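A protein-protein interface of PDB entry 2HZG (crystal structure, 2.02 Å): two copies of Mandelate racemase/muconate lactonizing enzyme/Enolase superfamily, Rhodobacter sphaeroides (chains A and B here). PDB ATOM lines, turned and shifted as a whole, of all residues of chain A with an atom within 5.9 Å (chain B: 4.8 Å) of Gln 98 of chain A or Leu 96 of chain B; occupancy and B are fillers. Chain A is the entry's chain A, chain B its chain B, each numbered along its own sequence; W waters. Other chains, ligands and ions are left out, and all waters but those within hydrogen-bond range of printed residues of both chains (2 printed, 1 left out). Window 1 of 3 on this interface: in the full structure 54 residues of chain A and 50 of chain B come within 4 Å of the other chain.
Water W1 lies within hydrogen-bond range of NE2 of Gln 98 of chain B (3.0 Å) and N of Leu 97 of chain A (3.1 Å).
Water W2 bridges the backbone carbonyl oxygen of Ala 46 of chain A (3.4 Å) and the side-chain sulfur of Cys 64 of chain B (3.7 Å).
Of chain B, only Leu 96 (3.9 Å), Leu 97 (3.4 Å) and Gln 98 (2.8 Å) come within 4 Å of Gln 98 of chain A.
Of chain A, only Ala 47, Pro 50 and Gln 98 come within 4 Å of Leu 96 of chain B.
Of the printed residues of chain A, Gln 98 of chain B touches Leu 96, Leu 97 and Gln 98.
Printed residues of chain B within 4 Å of Leu 97 of chain A: Leu 97 (3.2 Å), Gln 98 (3.5 Å) and Pro 100 (3.9 Å).
Printed residues of chain A within 4 Å of Leu 97 of chain B: Leu 97, Gln 98, Pro 100 and His 101.
Arg 65 of chain B touches none of the printed residues of chain A.
Ala 46 of chain A touches none of the printed residues of chain B.
The nearest printed residue of chain B that does not touch Gln 98 of chain A is Ala 99 of chain B (5.3 Å).
The nearest residue of chain A that does not touch Leu 96 of chain B is His 101 of chain A (5.4 Å).
The nearest printed residue of chain B that does not touch Leu 97 of chain A is Ala 99 of chain B (4.9 Å).
The backbone carbonyl oxygen (O) of Asp 95 of chain B is in hydrogen-bond range of the side-chain sulfur (SG) of Cys 64 of chain B, at 3.8 Å.
The side-chain hydroxyl of Ser 51 of chain A is in hydrogen-bond range of the backbone carbonyl oxygen of Ala 47 of chain A.
The backbone NH of Val 67 of chain B is in hydrogen-bond range of the backbone carbonyl oxygen of Ala 54 of chain B (2.9 Å).
The backbone NH of Asp 95 of chain B lies within hydrogen-bond range of the backbone carbonyl oxygen of Val 63 of chain B, 3.0 Å away.
NE2 of Gln 98 of chain A lies within hydrogen-bond range of OG of Ser 51 of chain A (3.0 Å).
Leu 96 of chain A touches Gln 98 of chain B, and with the chains exchanged Gln 98 of chain A touches Leu 96 of chain B.
Leu 97 of chain A touches its own counterpart, Leu 97 of chain B.
Leu 97 of chain A touches Gln 98 of chain B, and with the chains exchanged Gln 98 of chain A touches Leu 97 of chain B.
Gln 98 of chain B touches its own counterpart, Gln 98 of chain A.
Of the 15 pairs that touch across the chains among the printed residues, 8 have their exchanged pair printed and touching as well.
OE1 of Gln 98 of chain A lies within hydrogen-bond range of N of Gln 98 of chain B.
OE1 of Gln 98 of chain A sits close to N of Leu 97 of chain B (3.5 Å).
Printed residues of chain A that touch a printed residue of chain B: Ala 47, Pro 50, Leu 96, Leu 97, Gln 98, Pro 100 and His 101.
Hydrophobic or aromatic side chains of chain A within 4 Å of the printed part of chain B: Ala 47, Pro 50, Leu 96, Leu 97, Pro 100 and His 101.
Along chain A the printed residues that touch a printed residue of chain B span positions 47 to 101.
Printed residues of chain B that touch a printed residue of chain A: Ala 54, Cys 57, Cys 64, Asp 95, Leu 96, Leu 97, Gln 98 and Pro 100.
Among the printed residues, 15 pairs touch across the chains.
Among the printed residues, no Asp or Glu carboxylate lies within 4 Å of a Lys or Arg side-chain nitrogen of the other chain.
Ala 47 of chain A touches Leu 96 of chain B.
Pro 50 of chain A touches Ala 54 of chain B.
Pro 50 of chain A touches Cys 57 of chain B.
CD2 of Leu 96 of chain B touches CG of Pro 50 of chain A (3.8 Å).
OE1 of Gln 98 of chain B touches CD1 of Leu 96 of chain A (3.9 Å).
Leu 97 of chain A touches Leu 97 of chain B.
N of Leu 97 of chain A touches OE1 of Gln 98 of chain B, 3.5 Å away.
CD of Pro 100 of chain B touches CD2 of Leu 97 of chain A, at 3.9 Å.
CD2 of Leu 96 of chain B touches OE1 of Gln 98 of chain A, at 3.9 Å.
His 101 of chain A touches Asp 95 of chain B.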
ATOM      1  N   ALA A  46      18.367 -10.062  18.506  1.00  0.00           N
ATOM      2  CA  ALA A  46      17.593  -8.958  19.025  1.00  0.00           C
ATOM      3  C   ALA A  46      18.146  -7.704  18.410  1.00  0.00           C
ATOM      4  O   ALA A  46      19.270  -7.710  17.887  1.00  0.00           O
ATOM      5  CB  ALA A  46      17.760  -8.885  20.541  1.00  0.00           C
ATOM      6  N   ALA A  47      17.396  -6.616  18.555  1.00  0.00           N
ATOM      7  CA  ALA A  47      17.858  -5.289  18.159  1.00  0.00           C
ATOM      8  C   ALA A  47      18.989  -4.893  19.104  1.00  0.00           C
ATOM      9  O   ALA A  47      18.781  -4.801  20.311  1.00  0.00           O
ATOM     10  CB  ALA A  47      16.689  -4.281  18.214  1.00  0.00           C
ATOM     11  N   PRO A  50      18.633  -1.237  21.449  1.00  0.00           N
ATOM     12  CA  PRO A  50      17.658  -1.386  22.545  1.00  0.00           C
ATOM     13  C   PRO A  50      18.099  -2.403  23.583  1.00  0.00           C
ATOM     14  O   PRO A  50      17.855  -2.203  24.774  1.00  0.00           O
ATOM     15  CB  PRO A  50      16.396  -1.872  21.821  1.00  0.00           C
ATOM     16  CG  PRO A  50      16.509  -1.282  20.455  1.00  0.00           C
ATOM     17  CD  PRO A  50      17.997  -1.453  20.139  1.00  0.00           C
ATOM     18  N   SER A  51      18.745  -3.491  23.143  1.00  0.00           N
ATOM     19  CA  SER A  51      19.284  -4.482  24.070  1.00  0.00           C
ATOM     20  C   SER A  51      20.406  -3.902  24.926  1.00  0.00           C
ATOM     21  O   SER A  51      20.388  -4.073  26.143  1.00  0.00           O
ATOM     22  CB  SER A  51      19.765  -5.740  23.332  1.00  0.00           C
ATOM     23  OG  SER A  51      18.691  -6.318  22.623  1.00  0.00           O
ATOM     24  N   ALA A  54      18.832  -1.725  27.467  1.00  0.00           N
ATOM     25  CA  ALA A  54      18.304  -2.567  28.548  1.00  0.00           C
ATOM     26  C   ALA A  54      19.395  -2.988  29.543  1.00  0.00           C
ATOM     27  O   ALA A  54      19.143  -3.104  30.738  1.00  0.00           O
ATOM     28  CB  ALA A  54      17.541  -3.825  27.980  1.00  0.00           C
ATOM     29  N   LEU A  96      10.926  -3.955  32.224  1.00  0.00           N
ATOM     30  CA  LEU A  96      11.799  -3.577  31.128  1.00  0.00           C
ATOM     31  C   LEU A  96      11.545  -4.596  30.020  1.00  0.00           C
ATOM     32  O   LEU A  96      12.091  -5.709  30.034  1.00  0.00           O
ATOM     33  CB  LEU A  96      13.258  -3.542  31.619  1.00  0.00           C
ATOM     34  CG  LEU A  96      14.459  -3.439  30.670  1.00  0.00           C
ATOM     35  CD1 LEU A  96      14.148  -2.680  29.386  1.00  0.00           C
ATOM     36  CD2 LEU A  96      15.684  -2.875  31.395  1.00  0.00           C
ATOM     37  N   LEU A  97      10.672  -4.228  29.080  1.00  0.00           N
ATOM     38  CA  LEU A  97      10.168  -5.191  28.086  1.00  0.00           C
ATOM     39  C   LEU A  97      11.289  -5.880  27.291  1.00  0.00           C
ATOM     40  O   LEU A  97      11.222  -7.084  27.046  1.00  0.00           O
ATOM     41  CB  LEU A  97       9.142  -4.519  27.150  1.00  0.00           C
ATOM     42  CG  LEU A  97       8.462  -5.367  26.051  1.00  0.00           C
ATOM     43  CD1 LEU A  97       7.858  -6.645  26.606  1.00  0.00           C
ATOM     44  CD2 LEU A  97       7.393  -4.509  25.272  1.00  0.00           C
ATOM     45  N   GLN A  98      12.313  -5.119  26.921  1.00  0.00           N
ATOM     46  CA  GLN A  98      13.459  -5.631  26.150  1.00  0.00           C
ATOM     47  C   GLN A  98      14.299  -6.677  26.906  1.00  0.00           C
ATOM     48  O   GLN A  98      15.068  -7.418  26.271  1.00  0.00           O
ATOM     49  CB  GLN A  98      14.381  -4.469  25.730  1.00  0.00           C
ATOM     50  CG  GLN A  98      15.485  -4.825  24.708  1.00  0.00           C
ATOM     51  CD  GLN A  98      14.951  -5.074  23.295  1.00  0.00           C
ATOM     52  OE1 GLN A  98      13.836  -4.689  22.972  1.00  0.00           O
ATOM     53  NE2 GLN A  98      15.757  -5.705  22.448  1.00  0.00           N
ATOM     54  N   ALA A  99      14.148  -6.757  28.234  1.00  0.00           N
ATOM     55  CA  ALA A  99      15.085  -7.552  29.055  1.00  0.00           C
ATOM     56  C   ALA A  99      15.406  -8.996  28.562  1.00  0.00           C
ATOM     57  O   ALA A  99      16.573  -9.364  28.522  1.00  0.00           O
ATOM     58  CB  ALA A  99      14.684  -7.556  30.530  1.00  0.00           C
ATOM     59  N   PRO A 100      14.386  -9.811  28.207  1.00  0.00           N
ATOM     60  CA  PRO A 100      14.662 -11.205  27.833  1.00  0.00           C
ATOM     61  C   PRO A 100      15.638 -11.334  26.653  1.00  0.00           C
ATOM     62  O   PRO A 100      16.388 -12.300  26.596  1.00  0.00           O
ATOM     63  CB  PRO A 100      13.290 -11.731  27.397  1.00  0.00           C
ATOM     64  CG  PRO A 100      12.318 -10.844  28.004  1.00  0.00           C
ATOM     65  CD  PRO A 100      12.943  -9.516  28.165  1.00  0.00           C
ATOM     66  N   HIS A 101      15.610 -10.372  25.728  1.00  0.00           N
ATOM     67  CA  HIS A 101      16.473 -10.416  24.544  1.00  0.00           C
ATOM     68  C   HIS A 101      17.921 -10.140  24.927  1.00  0.00           C
ATOM     69  O   HIS A 101      18.836 -10.817  24.445  1.00  0.00           O
ATOM     70  CB  HIS A 101      15.968  -9.413  23.503  1.00  0.00           C
ATOM     71  CG  HIS A 101      14.882  -9.963  22.631  1.00  0.00           C
ATOM     72  ND1 HIS A 101      14.480  -9.351  21.460  1.00  0.00           N
ATOM     73  CD2 HIS A 101      14.132 -11.081  22.747  1.00  0.00           C
ATOM     74  CE1 HIS A 101      13.525 -10.071  20.898  1.00  0.00           C
ATOM     75  NE2 HIS A 101      13.302 -11.131  21.655  1.00  0.00           N
ATOM     76  N   MET A 102      18.118  -9.165  25.815  1.00  0.00           N
ATOM     77  CA  MET A 102      19.432  -8.880  26.395  1.00  0.00           C
ATOM     78  C   MET A 102      19.908 -10.072  27.239  1.00  0.00           C
ATOM     79  O   MET A 102      21.047 -10.528  27.097  1.00  0.00           O
ATOM     80  CB  MET A 102      19.391  -7.585  27.233  1.00  0.00           C
ATOM     81  CG  MET A 102      20.793  -7.116  27.733  1.00  0.00           C
ATOM     82  SD  MET A 102      21.975  -6.768  26.396  1.00  0.00           S
ATOM     83  CE  MET A 102      23.071  -8.166  26.479  1.00  0.00           C
ATOM     84  N   LEU A 103      19.026 -10.597  28.085  1.00  0.00           N
ATOM     85  CA  LEU A 103      19.347 -11.778  28.887  1.00  0.00           C
ATOM     86  C   LEU A 103      19.788 -13.008  28.070  1.00  0.00           C
ATOM     87  O   LEU A 103      20.678 -13.741  28.486  1.00  0.00           O
ATOM     88  CB  LEU A 103      18.164 -12.170  29.763  1.00  0.00           C
ATOM     89  CG  LEU A 103      18.292 -13.448  30.614  1.00  0.00           C
ATOM     90  CD1 LEU A 103      19.476 -13.363  31.635  1.00  0.00           C
ATOM     91  CD2 LEU A 103      16.988 -13.689  31.335  1.00  0.00           C
ATOM     92  N   ALA B  54      14.508   2.029  21.048  1.00  0.00           N
ATOM     93  CA  ALA B  54      13.540   1.437  20.134  1.00  0.00           C
ATOM     94  C   ALA B  54      13.069   2.410  19.056  1.00  0.00           C
ATOM     95  O   ALA B  54      12.796   2.012  17.932  1.00  0.00           O
ATOM     96  CB  ALA B  54      12.316   0.866  20.918  1.00  0.00           C
ATOM     97  N   CYS B  57      16.944   3.488  16.913  1.00  0.00           N
ATOM     98  CA  CYS B  57      18.026   2.539  16.612  1.00  0.00           C
ATOM     99  C   CYS B  57      18.216   2.311  15.116  1.00  0.00           C
ATOM    100  O   CYS B  57      17.267   2.392  14.342  1.00  0.00           O
ATOM    101  CB  CYS B  57      17.787   1.169  17.300  1.00  0.00           C
ATOM    102  SG  CYS B  57      16.255   0.305  16.809  1.00  0.00           S
ATOM    103  N   VAL B  63      12.176  -6.406   9.418  1.00  0.00           N
ATOM    104  CA  VAL B  63      11.150  -6.504  10.476  1.00  0.00           C
ATOM    105  C   VAL B  63      11.740  -6.236  11.857  1.00  0.00           C
ATOM    106  O   VAL B  63      11.170  -6.594  12.894  1.00  0.00           O
ATOM    107  CB  VAL B  63      10.245  -7.805  10.384  1.00  0.00           C
ATOM    108  CG1 VAL B  63       9.475  -7.815   9.075  1.00  0.00           C
ATOM    109  CG2 VAL B  63      11.051  -9.107  10.511  1.00  0.00           C
ATOM    110  N   CYS B  64      12.899  -5.586  11.850  1.00  0.00           N
ATOM    111  CA  CYS B  64      13.464  -5.019  13.056  1.00  0.00           C
ATOM    112  C   CYS B  64      13.921  -3.584  12.776  1.00  0.00           C
ATOM    113  O   CYS B  64      15.100  -3.260  12.881  1.00  0.00           O
ATOM    114  CB  CYS B  64      14.628  -5.878  13.570  1.00  0.00           C
ATOM    115  SG  CYS B  64      15.063  -5.528  15.299  1.00  0.00           S
ATOM    116  N   ARG B  65      12.974  -2.736  12.389  1.00  0.00           N
ATOM    117  CA  ARG B  65      13.242  -1.334  12.148  1.00  0.00           C
ATOM    118  C   ARG B  65      12.983  -0.459  13.390  1.00  0.00           C
ATOM    119  O   ARG B  65      12.161  -0.795  14.240  1.00  0.00           O
ATOM    120  CB  ARG B  65      12.373  -0.829  10.991  1.00  0.00           C
ATOM    121  CG  ARG B  65      12.574  -1.575   9.698  1.00  0.00           C
ATOM    122  CD  ARG B  65      11.714  -0.959   8.603  1.00  0.00           C
ATOM    123  NE  ARG B  65      11.353  -1.972   7.624  1.00  0.00           N
ATOM    124  CZ  ARG B  65      10.850  -1.716   6.422  1.00  0.00           C
ATOM    125  NH1 ARG B  65      10.654  -0.454   6.042  1.00  0.00           N
ATOM    126  NH2 ARG B  65      10.545  -2.725   5.606  1.00  0.00           N
ATOM    127  N   PRO B  66      13.655   0.697  13.472  1.00  0.00           N
ATOM    128  CA  PRO B  66      13.349   1.629  14.550  1.00  0.00           C
ATOM    129  C   PRO B  66      11.847   1.982  14.450  1.00  0.00           C
ATOM    130  O   PRO B  66      11.270   1.933  13.348  1.00  0.00           O
ATOM    131  CB  PRO B  66      14.204   2.850  14.204  1.00  0.00           C
ATOM    132  CG  PRO B  66      14.452   2.741  12.724  1.00  0.00           C
ATOM    133  CD  PRO B  66      14.658   1.248  12.544  1.00  0.00           C
ATOM    134  N   VAL B  67      11.210   2.297  15.578  1.00  0.00           N
ATOM    135  CA  VAL B  67       9.790   2.677  15.563  1.00  0.00           C
ATOM    136  C   VAL B  67       9.565   3.915  14.678  1.00  0.00           C
ATOM    137  O   VAL B  67       8.536   4.030  14.006  1.00  0.00           O
ATOM    138  CB  VAL B  67       9.220   2.847  16.995  1.00  0.00           C
ATOM    139  CG1 VAL B  67       7.769   3.359  16.960  1.00  0.00           C
ATOM    140  CG2 VAL B  67       9.307   1.497  17.776  1.00  0.00           C
ATOM    141  N   SER B  93       8.579  -3.570  13.117  1.00  0.00           N
ATOM    142  CA  SER B  93       9.327  -3.643  14.388  1.00  0.00           C
ATOM    143  C   SER B  93       8.997  -4.910  15.173  1.00  0.00           C
ATOM    144  O   SER B  93       9.209  -4.975  16.385  1.00  0.00           O
ATOM    145  CB  SER B  93       9.029  -2.402  15.230  1.00  0.00           C
ATOM    146  OG  SER B  93       9.562  -1.250  14.617  1.00  0.00           O
ATOM    147  N   MET B  94       8.486  -5.926  14.484  1.00  0.00           N
ATOM    148  CA  MET B  94       8.068  -7.162  15.149  1.00  0.00           C
ATOM    149  C   MET B  94       9.168  -7.816  15.990  1.00  0.00           C
ATOM    150  O   MET B  94       8.879  -8.368  17.059  1.00  0.00           O
ATOM    151  CB  MET B  94       7.443  -8.172  14.166  1.00  0.00           C
ATOM    152  CG  MET B  94       8.395  -9.101  13.428  1.00  0.00           C
ATOM    153  SD  MET B  94       7.542 -10.519  12.660  1.00  0.00           S
ATOM    154  CE  MET B  94       6.696  -9.708  11.357  1.00  0.00           C
ATOM    155  N   ASP B  95      10.417  -7.719  15.528  1.00  0.00           N
ATOM    156  CA  ASP B  95      11.563  -8.327  16.235  1.00  0.00           C
ATOM    157  C   ASP B  95      12.281  -7.384  17.209  1.00  0.00           C
ATOM    158  O   ASP B  95      13.313  -7.728  17.800  1.00  0.00           O
ATOM    159  CB  ASP B  95      12.546  -8.901  15.220  1.00  0.00           C
ATOM    160  CG  ASP B  95      12.031 -10.186  14.590  1.00  0.00           C
ATOM    161  OD1 ASP B  95      11.128 -10.843  15.161  1.00  0.00           O
ATOM    162  OD2 ASP B  95      12.563 -10.564  13.544  1.00  0.00           O
ATOM    163  N   LEU B  96      11.727  -6.186  17.356  1.00  0.00           N
ATOM    164  CA  LEU B  96      12.256  -5.213  18.287  1.00  0.00           C
ATOM    165  C   LEU B  96      11.343  -5.326  19.514  1.00  0.00           C
ATOM    166  O   LEU B  96      10.222  -4.804  19.527  1.00  0.00           O
ATOM    167  CB  LEU B  96      12.265  -3.815  17.653  1.00  0.00           C
ATOM    168  CG  LEU B  96      13.160  -2.720  18.270  1.00  0.00           C
ATOM    169  CD1 LEU B  96      12.819  -1.404  17.594  1.00  0.00           C
ATOM    170  CD2 LEU B  96      13.007  -2.590  19.809  1.00  0.00           C
ATOM    171  N   LEU B  97      11.815  -6.052  20.529  1.00  0.00           N
ATOM    172  CA  LEU B  97      10.958  -6.434  21.644  1.00  0.00           C
ATOM    173  C   LEU B  97      10.304  -5.263  22.390  1.00  0.00           C
ATOM    174  O   LEU B  97       9.123  -5.343  22.757  1.00  0.00           O
ATOM    175  CB  LEU B  97      11.703  -7.343  22.619  1.00  0.00           C
ATOM    176  CG  LEU B  97      10.896  -7.977  23.759  1.00  0.00           C
ATOM    177  CD1 LEU B  97       9.612  -8.666  23.265  1.00  0.00           C
ATOM    178  CD2 LEU B  97      11.800  -8.972  24.550  1.00  0.00           C
ATOM    179  N   GLN B  98      11.075  -4.206  22.605  1.00  0.00           N
ATOM    180  CA  GLN B  98      10.629  -2.994  23.294  1.00  0.00           C
ATOM    181  C   GLN B  98       9.524  -2.217  22.558  1.00  0.00           C
ATOM    182  O   GLN B  98       8.818  -1.419  23.170  1.00  0.00           O
ATOM    183  CB  GLN B  98      11.827  -2.066  23.512  1.00  0.00           C
ATOM    184  CG  GLN B  98      11.542  -0.851  24.433  1.00  0.00           C
ATOM    185  CD  GLN B  98      11.417  -1.234  25.917  1.00  0.00           C
ATOM    186  OE1 GLN B  98      11.792  -2.334  26.320  1.00  0.00           O
ATOM    187  NE2 GLN B  98      10.879  -0.316  26.731  1.00  0.00           N
ATOM    188  N   ALA B  99       9.378  -2.452  21.254  1.00  0.00           N
ATOM    189  CA  ALA B  99       8.537  -1.593  20.416  1.00  0.00           C
ATOM    190  C   ALA B  99       7.115  -1.238  20.945  1.00  0.00           C
ATOM    191  O   ALA B  99       6.747  -0.067  20.924  1.00  0.00           O
ATOM    192  CB  ALA B  99       8.536  -2.058  18.956  1.00  0.00           C
ATOM    193  N   PRO B 100       6.339  -2.228  21.461  1.00  0.00           N
ATOM    194  CA  PRO B 100       4.978  -1.949  21.994  1.00  0.00           C
ATOM    195  C   PRO B 100       4.916  -0.864  23.069  1.00  0.00           C
ATOM    196  O   PRO B 100       3.964  -0.064  23.102  1.00  0.00           O
ATOM    197  CB  PRO B 100       4.552  -3.297  22.575  1.00  0.00           C
ATOM    198  CG  PRO B 100       5.287  -4.284  21.705  1.00  0.00           C
ATOM    199  CD  PRO B 100       6.641  -3.671  21.530  1.00  0.00           C
HETATM  200  O   HOH W   1       9.634  -1.366  29.295  1.00  0.00           O
HETATM  201  O   HOH W   2      17.212  -8.540  15.359  1.00  0.00           O
